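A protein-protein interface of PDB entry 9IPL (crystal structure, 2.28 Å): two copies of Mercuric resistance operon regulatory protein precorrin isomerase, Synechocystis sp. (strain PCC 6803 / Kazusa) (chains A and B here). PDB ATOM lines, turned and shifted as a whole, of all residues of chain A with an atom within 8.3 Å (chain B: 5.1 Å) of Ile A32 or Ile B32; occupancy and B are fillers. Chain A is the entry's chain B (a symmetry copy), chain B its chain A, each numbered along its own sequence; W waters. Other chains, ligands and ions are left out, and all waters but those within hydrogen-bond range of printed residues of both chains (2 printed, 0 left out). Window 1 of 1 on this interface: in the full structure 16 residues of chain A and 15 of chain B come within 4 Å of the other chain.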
ATOM      1  N   PHE A  13      16.060  10.168 -26.699  1.00  0.00           N
ATOM      2  CA  PHE A  13      16.691  11.480 -26.766  1.00  0.00           C
ATOM      3  C   PHE A  13      16.954  11.847 -28.226  1.00  0.00           C
ATOM      4  O   PHE A  13      16.354  12.793 -28.735  1.00  0.00           O
ATOM      5  CB  PHE A  13      18.003  11.556 -25.975  1.00  0.00           C
ATOM      6  N   GLN A  14      17.824  11.068 -28.890  1.00  0.00           N
ATOM      7  CA  GLN A  14      18.350  11.410 -30.207  1.00  0.00           C
ATOM      8  C   GLN A  14      17.221  11.669 -31.209  1.00  0.00           C
ATOM      9  O   GLN A  14      17.318  12.587 -32.022  1.00  0.00           O
ATOM     10  CB  GLN A  14      19.296  10.310 -30.686  1.00  0.00           C
ATOM     11  N   LEU A  17      15.106  14.908 -30.259  1.00  0.00           N
ATOM     12  CA  LEU A  17      15.919  16.080 -30.553  1.00  0.00           C
ATOM     13  C   LEU A  17      15.813  16.395 -32.041  1.00  0.00           C
ATOM     14  O   LEU A  17      15.579  17.539 -32.406  1.00  0.00           O
ATOM     15  CB  LEU A  17      17.375  15.915 -30.104  1.00  0.00           C
ATOM     16  CG  LEU A  17      17.615  15.688 -28.601  1.00  0.00           C
ATOM     17  CD1 LEU A  17      19.092  15.483 -28.297  1.00  0.00           C
ATOM     18  CD2 LEU A  17      17.063  16.790 -27.704  1.00  0.00           C
ATOM     19  N   LYS A  18      15.929  15.367 -32.885  1.00  0.00           N
ATOM     20  CA  LYS A  18      15.803  15.535 -34.325  1.00  0.00           C
ATOM     21  C   LYS A  18      14.568  16.380 -34.659  1.00  0.00           C
ATOM     22  O   LYS A  18      14.698  17.402 -35.325  1.00  0.00           O
ATOM     23  CB  LYS A  18      15.821  14.167 -35.021  1.00  0.00           C
ATOM     24  N   LEU A  20      12.586  18.187 -32.733  1.00  0.00           N
ATOM     25  CA  LEU A  20      12.364  19.374 -31.909  1.00  0.00           C
ATOM     26  C   LEU A  20      13.272  20.542 -32.295  1.00  0.00           C
ATOM     27  O   LEU A  20      13.069  21.647 -31.811  1.00  0.00           O
ATOM     28  CB  LEU A  20      12.549  19.048 -30.427  1.00  0.00           C
ATOM     29  CG  LEU A  20      11.479  18.166 -29.783  1.00  0.00           C
ATOM     30  CD1 LEU A  20      11.884  17.907 -28.352  1.00  0.00           C
ATOM     31  CD2 LEU A  20      10.096  18.805 -29.845  1.00  0.00           C
ATOM     32  N   LEU A  21      14.272  20.316 -33.151  1.00  0.00           N
ATOM     33  CA  LEU A  21      15.222  21.367 -33.489  1.00  0.00           C
ATOM     34  C   LEU A  21      14.641  22.361 -34.490  1.00  0.00           C
ATOM     35  O   LEU A  21      14.996  23.542 -34.457  1.00  0.00           O
ATOM     36  CB  LEU A  21      16.533  20.771 -34.003  1.00  0.00           C
ATOM     37  CG  LEU A  21      17.398  20.074 -32.949  1.00  0.00           C
ATOM     38  CD1 LEU A  21      18.573  19.433 -33.624  1.00  0.00           C
ATOM     39  CD2 LEU A  21      17.853  21.011 -31.839  1.00  0.00           C
ATOM     40  N   ASP A  26      11.649  26.196 -27.118  1.00  0.00           N
ATOM     41  CA  ASP A  26      12.890  25.655 -26.572  1.00  0.00           C
ATOM     42  C   ASP A  26      12.713  24.242 -26.013  1.00  0.00           C
ATOM     43  O   ASP A  26      13.302  23.905 -24.988  1.00  0.00           O
ATOM     44  CB  ASP A  26      13.471  26.574 -25.510  1.00  0.00           C
ATOM     45  CG  ASP A  26      13.934  27.928 -26.028  1.00  0.00           C
ATOM     46  OD1 ASP A  26      14.729  27.954 -27.011  1.00  0.00           O
ATOM     47  OD2 ASP A  26      13.507  28.940 -25.434  1.00  0.00           O
ATOM     48  N   TYR A  27      11.977  23.380 -26.715  1.00  0.00           N
ATOM     49  CA  TYR A  27      11.664  22.073 -26.168  1.00  0.00           C
ATOM     50  C   TYR A  27      12.895  21.171 -26.202  1.00  0.00           C
ATOM     51  O   TYR A  27      12.978  20.235 -25.405  1.00  0.00           O
ATOM     52  CB  TYR A  27      10.471  21.419 -26.869  1.00  0.00           C
ATOM     53  CG  TYR A  27       9.130  22.103 -26.636  1.00  0.00           C
ATOM     54  CD1 TYR A  27       8.952  23.043 -25.624  1.00  0.00           C
ATOM     55  CD2 TYR A  27       8.039  21.830 -27.457  1.00  0.00           C
ATOM     56  CE1 TYR A  27       7.738  23.681 -25.432  1.00  0.00           C
ATOM     57  CE2 TYR A  27       6.816  22.457 -27.271  1.00  0.00           C
ATOM     58  CZ  TYR A  27       6.665  23.377 -26.251  1.00  0.00           C
ATOM     59  OH  TYR A  27       5.467  23.992 -26.048  1.00  0.00           O
ATOM     60  N   SER A  28      13.820  21.424 -27.133  1.00  0.00           N
ATOM     61  CA  SER A  28      15.040  20.634 -27.233  1.00  0.00           C
ATOM     62  C   SER A  28      15.953  20.939 -26.043  1.00  0.00           C
ATOM     63  O   SER A  28      16.567  20.040 -25.482  1.00  0.00           O
ATOM     64  CB  SER A  28      15.757  20.885 -28.547  1.00  0.00           C
ATOM     65  OG  SER A  28      16.081  22.263 -28.691  1.00  0.00           O
ATOM     66  N   GLU A  29      16.043  22.214 -25.673  1.00  0.00           N
ATOM     67  CA  GLU A  29      16.852  22.639 -24.540  1.00  0.00           C
ATOM     68  C   GLU A  29      16.268  22.072 -23.242  1.00  0.00           C
ATOM     69  O   GLU A  29      17.015  21.657 -22.358  1.00  0.00           O
ATOM     70  CB  GLU A  29      16.922  24.163 -24.417  1.00  0.00           C
ATOM     71  CG  GLU A  29      17.729  24.865 -25.506  1.00  0.00           C
ATOM     72  CD  GLU A  29      16.994  25.227 -26.800  1.00  0.00           C
ATOM     73  OE1 GLU A  29      15.913  24.648 -27.094  1.00  0.00           O
ATOM     74  OE2 GLU A  29      17.507  26.134 -27.506  1.00  0.00           O
ATOM     75  N   ILE A  30      14.931  22.091 -23.127  1.00  0.00           N
ATOM     76  CA  ILE A  30      14.223  21.608 -21.951  1.00  0.00           C
ATOM     77  C   ILE A  30      14.423  20.105 -21.795  1.00  0.00           C
ATOM     78  O   ILE A  30      14.649  19.651 -20.679  1.00  0.00           O
ATOM     79  CB  ILE A  30      12.740  22.009 -21.994  1.00  0.00           C
ATOM     80  CG1 ILE A  30      12.600  23.519 -21.789  1.00  0.00           C
ATOM     81  CG2 ILE A  30      11.916  21.228 -20.962  1.00  0.00           C
ATOM     82  CD1 ILE A  30      11.193  24.056 -22.011  1.00  0.00           C
ATOM     83  N   THR A  31      14.406  19.362 -22.907  1.00  0.00           N
ATOM     84  CA  THR A  31      14.597  17.922 -22.883  1.00  0.00           C
ATOM     85  C   THR A  31      15.984  17.579 -22.341  1.00  0.00           C
ATOM     86  O   THR A  31      16.134  16.592 -21.622  1.00  0.00           O
ATOM     87  CB  THR A  31      14.415  17.343 -24.287  1.00  0.00           C
ATOM     88  OG1 THR A  31      13.094  17.650 -24.696  1.00  0.00           O
ATOM     89  CG2 THR A  31      14.624  15.842 -24.349  1.00  0.00           C
ATOM     90  N   ILE A  32      17.012  18.340 -22.743  1.00  0.00           N
ATOM     91  CA  ILE A  32      18.376  17.999 -22.364  1.00  0.00           C
ATOM     92  C   ILE A  32      18.625  18.439 -20.922  1.00  0.00           C
ATOM     93  O   ILE A  32      19.353  17.769 -20.201  1.00  0.00           O
ATOM     94  CB  ILE A  32      19.405  18.541 -23.373  1.00  0.00           C
ATOM     95  CG1 ILE A  32      19.533  17.567 -24.530  1.00  0.00           C
ATOM     96  CG2 ILE A  32      20.782  18.771 -22.759  1.00  0.00           C
ATOM     97  CD1 ILE A  32      20.423  16.375 -24.208  1.00  0.00           C
ATOM     98  N   HIS A  33      17.989  19.535 -20.504  1.00  0.00           N
ATOM     99  CA  HIS A  33      18.022  19.947 -19.114  1.00  0.00           C
ATOM    100  C   HIS A  33      17.463  18.836 -18.215  1.00  0.00           C
ATOM    101  O   HIS A  33      18.055  18.515 -17.196  1.00  0.00           O
ATOM    102  CB  HIS A  33      17.257  21.254 -18.922  1.00  0.00           C
ATOM    103  CG  HIS A  33      17.350  21.760 -17.535  1.00  0.00           C
ATOM    104  ND1 HIS A  33      18.577  22.010 -16.958  1.00  0.00           N
ATOM    105  CD2 HIS A  33      16.422  21.996 -16.586  1.00  0.00           C
ATOM    106  CE1 HIS A  33      18.379  22.437 -15.715  1.00  0.00           C
ATOM    107  NE2 HIS A  33      17.080  22.448 -15.470  1.00  0.00           N
ATOM    108  N   LEU A  34      16.332  18.246 -18.613  1.00  0.00           N
ATOM    109  CA  LEU A  34      15.701  17.184 -17.850  1.00  0.00           C
ATOM    110  C   LEU A  34      16.626  15.971 -17.758  1.00  0.00           C
ATOM    111  O   LEU A  34      16.846  15.463 -16.663  1.00  0.00           O
ATOM    112  CB  LEU A  34      14.344  16.847 -18.455  1.00  0.00           C
ATOM    113  CG  LEU A  34      13.546  15.760 -17.734  1.00  0.00           C
ATOM    114  CD1 LEU A  34      12.062  15.984 -17.862  1.00  0.00           C
ATOM    115  CD2 LEU A  34      13.905  14.420 -18.315  1.00  0.00           C
ATOM    116  N   LEU A  35      17.205  15.533 -18.881  1.00  0.00           N
ATOM    117  CA  LEU A  35      18.149  14.427 -18.868  1.00  0.00           C
ATOM    118  C   LEU A  35      19.336  14.709 -17.940  1.00  0.00           C
ATOM    119  O   LEU A  35      19.771  13.828 -17.189  1.00  0.00           O
ATOM    120  CB  LEU A  35      18.616  14.126 -20.290  1.00  0.00           C
ATOM    121  CG  LEU A  35      17.569  13.474 -21.200  1.00  0.00           C
ATOM    122  CD1 LEU A  35      18.018  13.399 -22.649  1.00  0.00           C
ATOM    123  CD2 LEU A  35      17.260  12.081 -20.700  1.00  0.00           C
ATOM    124  N   HIS A  36      19.870  15.930 -18.038  1.00  0.00           N
ATOM    125  CA  HIS A  36      20.999  16.378 -17.246  1.00  0.00           C
ATOM    126  C   HIS A  36      20.691  16.281 -15.746  1.00  0.00           C
ATOM    127  O   HIS A  36      21.507  15.782 -14.983  1.00  0.00           O
ATOM    128  CB  HIS A  36      21.348  17.808 -17.677  1.00  0.00           C
ATOM    129  CG  HIS A  36      22.539  18.398 -17.023  1.00  0.00           C
ATOM    130  ND1 HIS A  36      22.622  19.740 -16.716  1.00  0.00           N
ATOM    131  CD2 HIS A  36      23.675  17.843 -16.609  1.00  0.00           C
ATOM    132  CE1 HIS A  36      23.788  19.977 -16.138  1.00  0.00           C
ATOM    133  NE2 HIS A  36      24.444  18.838 -16.063  1.00  0.00           N
ATOM    134  N   GLN A  37      19.540  16.817 -15.326  1.00  0.00           N
ATOM    135  CA  GLN A  37      19.106  16.762 -13.943  1.00  0.00           C
ATOM    136  C   GLN A  37      18.963  15.312 -13.451  1.00  0.00           C
ATOM    137  O   GLN A  37      19.353  15.008 -12.332  1.00  0.00           O
ATOM    138  CB  GLN A  37      17.802  17.545 -13.795  1.00  0.00           C
ATOM    139  CG  GLN A  37      17.949  19.047 -13.986  1.00  0.00           C
ATOM    140  CD  GLN A  37      18.749  19.723 -12.889  1.00  0.00           C
ATOM    141  OE1 GLN A  37      19.954  19.945 -13.014  1.00  0.00           O
ATOM    142  NE2 GLN A  37      18.083  20.058 -11.798  1.00  0.00           N
ATOM    143  N   LEU A  38      18.432  14.407 -14.283  1.00  0.00           N
ATOM    144  CA  LEU A  38      18.296  13.010 -13.911  1.00  0.00           C
ATOM    145  C   LEU A  38      19.667  12.396 -13.694  1.00  0.00           C
ATOM    146  O   LEU A  38      19.856  11.603 -12.771  1.00  0.00           O
ATOM    147  CB  LEU A  38      17.521  12.192 -14.945  1.00  0.00           C
ATOM    148  CG  LEU A  38      16.039  12.531 -15.114  1.00  0.00           C
ATOM    149  CD1 LEU A  38      15.447  11.732 -16.249  1.00  0.00           C
ATOM    150  CD2 LEU A  38      15.231  12.262 -13.872  1.00  0.00           C
ATOM    151  N   VAL A  39      20.617  12.716 -14.570  1.00  0.00           N
ATOM    152  CA  VAL A  39      21.944  12.147 -14.439  1.00  0.00           C
ATOM    153  C   VAL A  39      22.643  12.702 -13.191  1.00  0.00           C
ATOM    154  O   VAL A  39      23.472  12.011 -12.602  1.00  0.00           O
ATOM    155  CB  VAL A  39      22.772  12.367 -15.717  1.00  0.00           C
ATOM    156  CG1 VAL A  39      24.244  12.031 -15.522  1.00  0.00           C
ATOM    157  CG2 VAL A  39      22.202  11.564 -16.883  1.00  0.00           C
ATOM    158  N   VAL A  48      19.963   8.516 -21.036  1.00  0.00           N
ATOM    159  CA  VAL A  48      19.809   9.126 -22.349  1.00  0.00           C
ATOM    160  C   VAL A  48      19.072   8.146 -23.271  1.00  0.00           C
ATOM    161  O   VAL A  48      18.210   8.558 -24.049  1.00  0.00           O
ATOM    162  CB  VAL A  48      21.153   9.599 -22.941  1.00  0.00           C
ATOM    163  CG1 VAL A  48      21.015  10.106 -24.378  1.00  0.00           C
ATOM    164  CG2 VAL A  48      21.772  10.683 -22.073  1.00  0.00           C
ATOM    165  N   LEU A  53      10.198  10.265 -23.976  1.00  0.00           N
ATOM    166  CA  LEU A  53       9.166  11.285 -23.930  1.00  0.00           C
ATOM    167  C   LEU A  53       8.218  11.075 -25.104  1.00  0.00           C
ATOM    168  O   LEU A  53       8.628  10.628 -26.167  1.00  0.00           O
ATOM    169  CB  LEU A  53       9.764  12.691 -23.951  1.00  0.00           C
ATOM    170  CG  LEU A  53      10.658  13.050 -22.761  1.00  0.00           C
ATOM    171  CD1 LEU A  53      12.086  12.557 -22.970  1.00  0.00           C
ATOM    172  CD2 LEU A  53      10.616  14.545 -22.474  1.00  0.00           C
ATOM    173  N   ILE A  58       6.188  17.725 -23.176  1.00  0.00           N
ATOM    174  CA  ILE A  58       6.659  18.996 -22.651  1.00  0.00           C
ATOM    175  C   ILE A  58       5.566  20.048 -22.771  1.00  0.00           C
ATOM    176  O   ILE A  58       5.286  20.758 -21.803  1.00  0.00           O
ATOM    177  CB  ILE A  58       7.953  19.411 -23.356  1.00  0.00           C
ATOM    178  CG1 ILE A  58       9.032  18.359 -23.090  1.00  0.00           C
ATOM    179  CG2 ILE A  58       8.370  20.821 -22.922  1.00  0.00           C
ATOM    180  CD1 ILE A  58      10.387  18.647 -23.703  1.00  0.00           C
ATOM    181  N   ALA A 201      12.424  19.726 -13.260  1.00  0.00           N
ATOM    182  CA  ALA A 201      13.108  20.263 -14.423  1.00  0.00           C
ATOM    183  C   ALA A 201      12.133  21.040 -15.313  1.00  0.00           C
ATOM    184  O   ALA A 201      12.520  22.047 -15.891  1.00  0.00           O
ATOM    185  CB  ALA A 201      13.803  19.149 -15.179  1.00  0.00           C
ATOM    186  N   THR A 205      12.120  25.468 -15.673  1.00  0.00           N
ATOM    187  CA  THR A 205      12.330  26.064 -16.987  1.00  0.00           C
ATOM    188  C   THR A 205      11.078  26.802 -17.451  1.00  0.00           C
ATOM    189  O   THR A 205      10.992  27.195 -18.608  1.00  0.00           O
ATOM    190  CB  THR A 205      12.727  24.998 -18.007  1.00  0.00           C
ATOM    191  OG1 THR A 205      11.649  24.060 -18.086  1.00  0.00           O
ATOM    192  CG2 THR A 205      14.069  24.379 -17.660  1.00  0.00           C
ATOM    193  N   LEU B  17      27.350  14.955 -25.628  1.00  0.00           N
ATOM    194  CA  LEU B  17      26.266  14.984 -24.654  1.00  0.00           C
ATOM    195  C   LEU B  17      26.515  13.920 -23.590  1.00  0.00           C
ATOM    196  O   LEU B  17      26.420  14.203 -22.398  1.00  0.00           O
ATOM    197  CB  LEU B  17      24.894  14.828 -25.318  1.00  0.00           C
ATOM    198  CG  LEU B  17      24.493  15.922 -26.318  1.00  0.00           C
ATOM    199  CD1 LEU B  17      23.205  15.589 -27.056  1.00  0.00           C
ATOM    200  CD2 LEU B  17      24.366  17.290 -25.659  1.00  0.00           C
ATOM    201  N   LEU B  21      26.909  15.204 -19.417  1.00  0.00           N
ATOM    202  CA  LEU B  21      25.752  15.100 -18.537  1.00  0.00           C
ATOM    203  C   LEU B  21      26.156  14.868 -17.084  1.00  0.00           C
ATOM    204  O   LEU B  21      25.451  15.324 -16.177  1.00  0.00           O
ATOM    205  CB  LEU B  21      24.799  14.008 -19.019  1.00  0.00           C
ATOM    206  CG  LEU B  21      24.024  14.320 -20.303  1.00  0.00           C
ATOM    207  CD1 LEU B  21      23.243  13.105 -20.719  1.00  0.00           C
ATOM    208  CD2 LEU B  21      23.100  15.505 -20.159  1.00  0.00           C
ATOM    209  N   SER B  28      25.861  20.841 -21.601  1.00  0.00           N
ATOM    210  CA  SER B  28      24.984  20.017 -22.417  1.00  0.00           C
ATOM    211  C   SER B  28      23.821  20.865 -22.950  1.00  0.00           C
ATOM    212  O   SER B  28      23.437  20.746 -24.101  1.00  0.00           O
ATOM    213  CB  SER B  28      24.484  18.822 -21.636  1.00  0.00           C
ATOM    214  OG  SER B  28      23.789  19.242 -20.464  1.00  0.00           O
ATOM    215  N   GLU B  29      23.278  21.730 -22.104  1.00  0.00           N
ATOM    216  CA  GLU B  29      22.193  22.616 -22.490  1.00  0.00           C
ATOM    217  C   GLU B  29      22.691  23.621 -23.540  1.00  0.00           C
ATOM    218  O   GLU B  29      21.969  23.927 -24.487  1.00  0.00           O
ATOM    219  CB  GLU B  29      21.624  23.389 -21.295  1.00  0.00           C
ATOM    220  CG  GLU B  29      20.840  22.552 -20.283  1.00  0.00           C
ATOM    221  CD  GLU B  29      21.644  21.872 -19.171  1.00  0.00           C
ATOM    222  OE1 GLU B  29      22.878  21.694 -19.307  1.00  0.00           O
ATOM    223  OE2 GLU B  29      21.023  21.520 -18.143  1.00  0.00           O
ATOM    224  N   ILE B  30      23.911  24.137 -23.341  1.00  0.00           N
ATOM    225  CA  ILE B  30      24.527  25.105 -24.232  1.00  0.00           C
ATOM    226  C   ILE B  30      24.781  24.489 -25.601  1.00  0.00           C
ATOM    227  O   ILE B  30      24.523  25.145 -26.606  1.00  0.00           O
ATOM    228  CB  ILE B  30      25.803  25.696 -23.610  1.00  0.00           C
ATOM    229  CG1 ILE B  30      25.447  26.582 -22.423  1.00  0.00           C
ATOM    230  CG2 ILE B  30      26.629  26.461 -24.648  1.00  0.00           C
ATOM    231  CD1 ILE B  30      26.647  27.045 -21.616  1.00  0.00           C
ATOM    232  N   THR B  31      25.228  23.224 -25.639  1.00  0.00           N
ATOM    233  CA  THR B  31      25.515  22.547 -26.890  1.00  0.00           C
ATOM    234  C   THR B  31      24.241  22.403 -27.724  1.00  0.00           C
ATOM    235  O   THR B  31      24.285  22.527 -28.948  1.00  0.00           O
ATOM    236  CB  THR B  31      26.121  21.179 -26.601  1.00  0.00           C
ATOM    237  OG1 THR B  31      27.328  21.418 -25.888  1.00  0.00           O
ATOM    238  CG2 THR B  31      26.407  20.366 -27.848  1.00  0.00           C
ATOM    239  N   ILE B  32      23.115  22.095 -27.073  1.00  0.00           N
ATOM    240  CA  ILE B  32      21.883  21.823 -27.796  1.00  0.00           C
ATOM    241  C   ILE B  32      21.251  23.145 -28.222  1.00  0.00           C
ATOM    242  O   ILE B  32      20.631  23.209 -29.275  1.00  0.00           O
ATOM    243  CB  ILE B  32      20.943  20.914 -26.972  1.00  0.00           C
ATOM    244  CG1 ILE B  32      21.314  19.469 -27.191  1.00  0.00           C
ATOM    245  CG2 ILE B  32      19.463  21.117 -27.290  1.00  0.00           C
ATOM    246  CD1 ILE B  32      20.784  18.922 -28.508  1.00  0.00           C
ATOM    247  N   HIS B  33      21.439  24.191 -27.417  1.00  0.00           N
ATOM    248  CA  HIS B  33      21.010  25.524 -27.788  1.00  0.00           C
ATOM    249  C   HIS B  33      21.702  25.961 -29.078  1.00  0.00           C
ATOM    250  O   HIS B  33      21.053  26.476 -29.980  1.00  0.00           O
ATOM    251  CB  HIS B  33      21.271  26.514 -26.655  1.00  0.00           C
ATOM    252  CG  HIS B  33      20.730  27.851 -26.958  1.00  0.00           C
ATOM    253  ND1 HIS B  33      19.391  28.027 -27.230  1.00  0.00           N
ATOM    254  CD2 HIS B  33      21.316  29.051 -27.107  1.00  0.00           C
ATOM    255  CE1 HIS B  33      19.170  29.312 -27.480  1.00  0.00           C
ATOM    256  NE2 HIS B  33      20.327  29.952 -27.398  1.00  0.00           N
ATOM    257  N   LEU B  34      23.014  25.723 -29.161  1.00  0.00           N
ATOM    258  CA  LEU B  34      23.792  26.073 -30.336  1.00  0.00           C
ATOM    259  C   LEU B  34      23.281  25.311 -31.558  1.00  0.00           C
ATOM    260  O   LEU B  34      23.040  25.921 -32.584  1.00  0.00           O
ATOM    261  CB  LEU B  34      25.277  25.837 -30.071  1.00  0.00           C
ATOM    262  CG  LEU B  34      26.225  26.150 -31.234  1.00  0.00           C
ATOM    263  CD1 LEU B  34      27.577  26.641 -30.772  1.00  0.00           C
ATOM    264  CD2 LEU B  34      26.409  24.908 -32.053  1.00  0.00           C
ATOM    265  N   LEU B  35      23.070  23.998 -31.444  1.00  0.00           N
ATOM    266  CA  LEU B  35      22.546  23.213 -32.554  1.00  0.00           C
ATOM    267  C   LEU B  35      21.179  23.734 -33.001  1.00  0.00           C
ATOM    268  O   LEU B  35      20.908  23.836 -34.197  1.00  0.00           O
ATOM    269  CB  LEU B  35      22.479  21.738 -32.159  1.00  0.00           C
ATOM    270  CG  LEU B  35      23.836  21.033 -32.047  1.00  0.00           C
ATOM    271  CD1 LEU B  35      23.738  19.645 -31.452  1.00  0.00           C
ATOM    272  CD2 LEU B  35      24.480  20.937 -33.414  1.00  0.00           C
ATOM    273  N   HIS B  36      20.327  24.042 -32.023  1.00  0.00           N
ATOM    274  CA  HIS B  36      18.982  24.536 -32.256  1.00  0.00           C
ATOM    275  C   HIS B  36      19.017  25.846 -33.056  1.00  0.00           C
ATOM    276  O   HIS B  36      18.279  26.001 -34.018  1.00  0.00           O
ATOM    277  CB  HIS B  36      18.286  24.688 -30.898  1.00  0.00           C
ATOM    278  CG  HIS B  36      16.865  25.098 -30.959  1.00  0.00           C
ATOM    279  ND1 HIS B  36      16.286  25.893 -29.995  1.00  0.00           N
ATOM    280  CD2 HIS B  36      15.906  24.840 -31.848  1.00  0.00           C
ATOM    281  CE1 HIS B  36      15.012  26.112 -30.304  1.00  0.00           C
ATOM    282  NE2 HIS B  36      14.758  25.480 -31.432  1.00  0.00           N
ATOM    283  N   GLN B  37      19.847  26.796 -32.626  1.00  0.00           N
ATOM    284  CA  GLN B  37      20.010  28.070 -33.309  1.00  0.00           C
ATOM    285  C   GLN B  37      20.520  27.879 -34.745  1.00  0.00           C
ATOM    286  O   GLN B  37      20.045  28.557 -35.651  1.00  0.00           O
ATOM    287  CB  GLN B  37      20.925  28.986 -32.495  1.00  0.00           C
ATOM    288  CG  GLN B  37      20.332  29.431 -31.162  1.00  0.00           C
ATOM    289  CD  GLN B  37      19.142  30.358 -31.299  1.00  0.00           C
ATOM    290  OE1 GLN B  37      17.992  29.933 -31.232  1.00  0.00           O
ATOM    291  NE2 GLN B  37      19.398  31.635 -31.523  1.00  0.00           N
HETATM  292  O   HOH W   1      13.513  23.083 -29.660  1.00  0.00           O
HETATM  293  O   HOH W   2      26.283  19.713 -18.874  1.00  0.00           O
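The side-chain carboxylate of Glu B29 lies within hydrogen-bond range of a ring nitrogen (ND1) of His A33 (2.8 Å).
OE2 of Glu B29 sits at hydrogen-bond distance from ND1 of His A36 (2.8 Å).
OE2 of Glu A29 sits at hydrogen-bond distance from ND1 of His B33.
The side-chain carboxylate (OE2) of Glu A29 is in hydrogen-bond range of a ring nitrogen (ND1) of His B36.
The side-chain carboxylate (OE1) of Glu B29 sits at hydrogen-bond distance from the side-chain hydroxyl (OG) of Ser B28, 2.9 Å away.
The side-chain hydroxyl of Ser A28 lies within hydrogen-bond range of the side-chain carboxylate of Glu A29 (2.9 Å).
Leu A21 touches His B36 (O to CD2, 3.1 Å).
OD1 of Asp A26 touches CE1 of His B36, at 3.8 Å.
Ser A28 touches His B36 (OG to CG, 3.7 Å).
Glu A29 touches Ile B32 (N to CG2, 3.9 Å).
Ser B28 touches Ile A32.
N of Glu B29 touches CG2 of Ile A32, 3.9 Å away.
Ile B32 touches Ile A32 (CG1 to CG1, 3.7 Å).
His A36 touches Leu B21 (CD2 to O, 3.1 Å).
Val A39 touches Leu B21.
Leu B21 touches Val A48 (CD1 to CG2, 3.1 Å).
Printed residues of chain B within 4 Å of Leu A17: Ile B32 (3.8 Å).
Of the printed residues of chain B, Glu A29 touches Ile B32 (3.9 Å), His B33 (2.7 Å) and His B36 (2.8 Å).
Ile A30 touches none of the printed residues of chain B.
Ile A32 touches just these residues of chain B: Ser B28 (3.6 Å), Glu B29 (3.9 Å) and Ile B32 (3.7 Å).
Printed residues of chain A within 4 Å of Leu B21: His A36 (3.1 Å), Val A39 (3.6 Å) and Val A48 (3.1 Å).
Ile B32 touches just these residues of chain A: Leu A17, Ser A28, Glu A29 and Ile A32.
The nearest printed residue of chain B that does not touch Val A48 is Leu B17 (5.8 Å).
Of the 12 printed residues of chain B, 6 touch a printed residue of chain A.
Printed residues of chain B that touch a printed residue of chain A: Leu B21, Ser B28, Glu B29, Ile B32, His B33 and His B36.
Of the 25 printed residues of chain A, 10 touch a printed residue of chain B.
Hydrophobic or aromatic side chains of chain A within 4 Å of the printed part of chain B: Leu A17, Leu A21, Ile A32, His A33, His A36, Val A39 and Val A48.
Among the printed residues, 17 pairs touch across the chains.
Leu A17 touches Ile B32, but with the chains exchanged Ile A32 does not touch Leu B17 (4.1 Å).
Leu A21 touches His B36, and with the chains exchanged His A36 touches Leu B21.
Ser A28 touches Ile B32, and with the chains exchanged Ile A32 touches Ser B28.
Ile B32 touches its own counterpart, Ile A32.
Of the 17 pairs that touch across the chains among the printed residues, 13 have their exchanged pair printed and touching as well.
Water W1 lies within hydrogen-bond range of O of Leu A20, OG of Ser A28, NE2 of His B36 and N of Tyr A27.
Water W2 lies within hydrogen-bond range of N of Ser B28 and NE2 of His A36.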
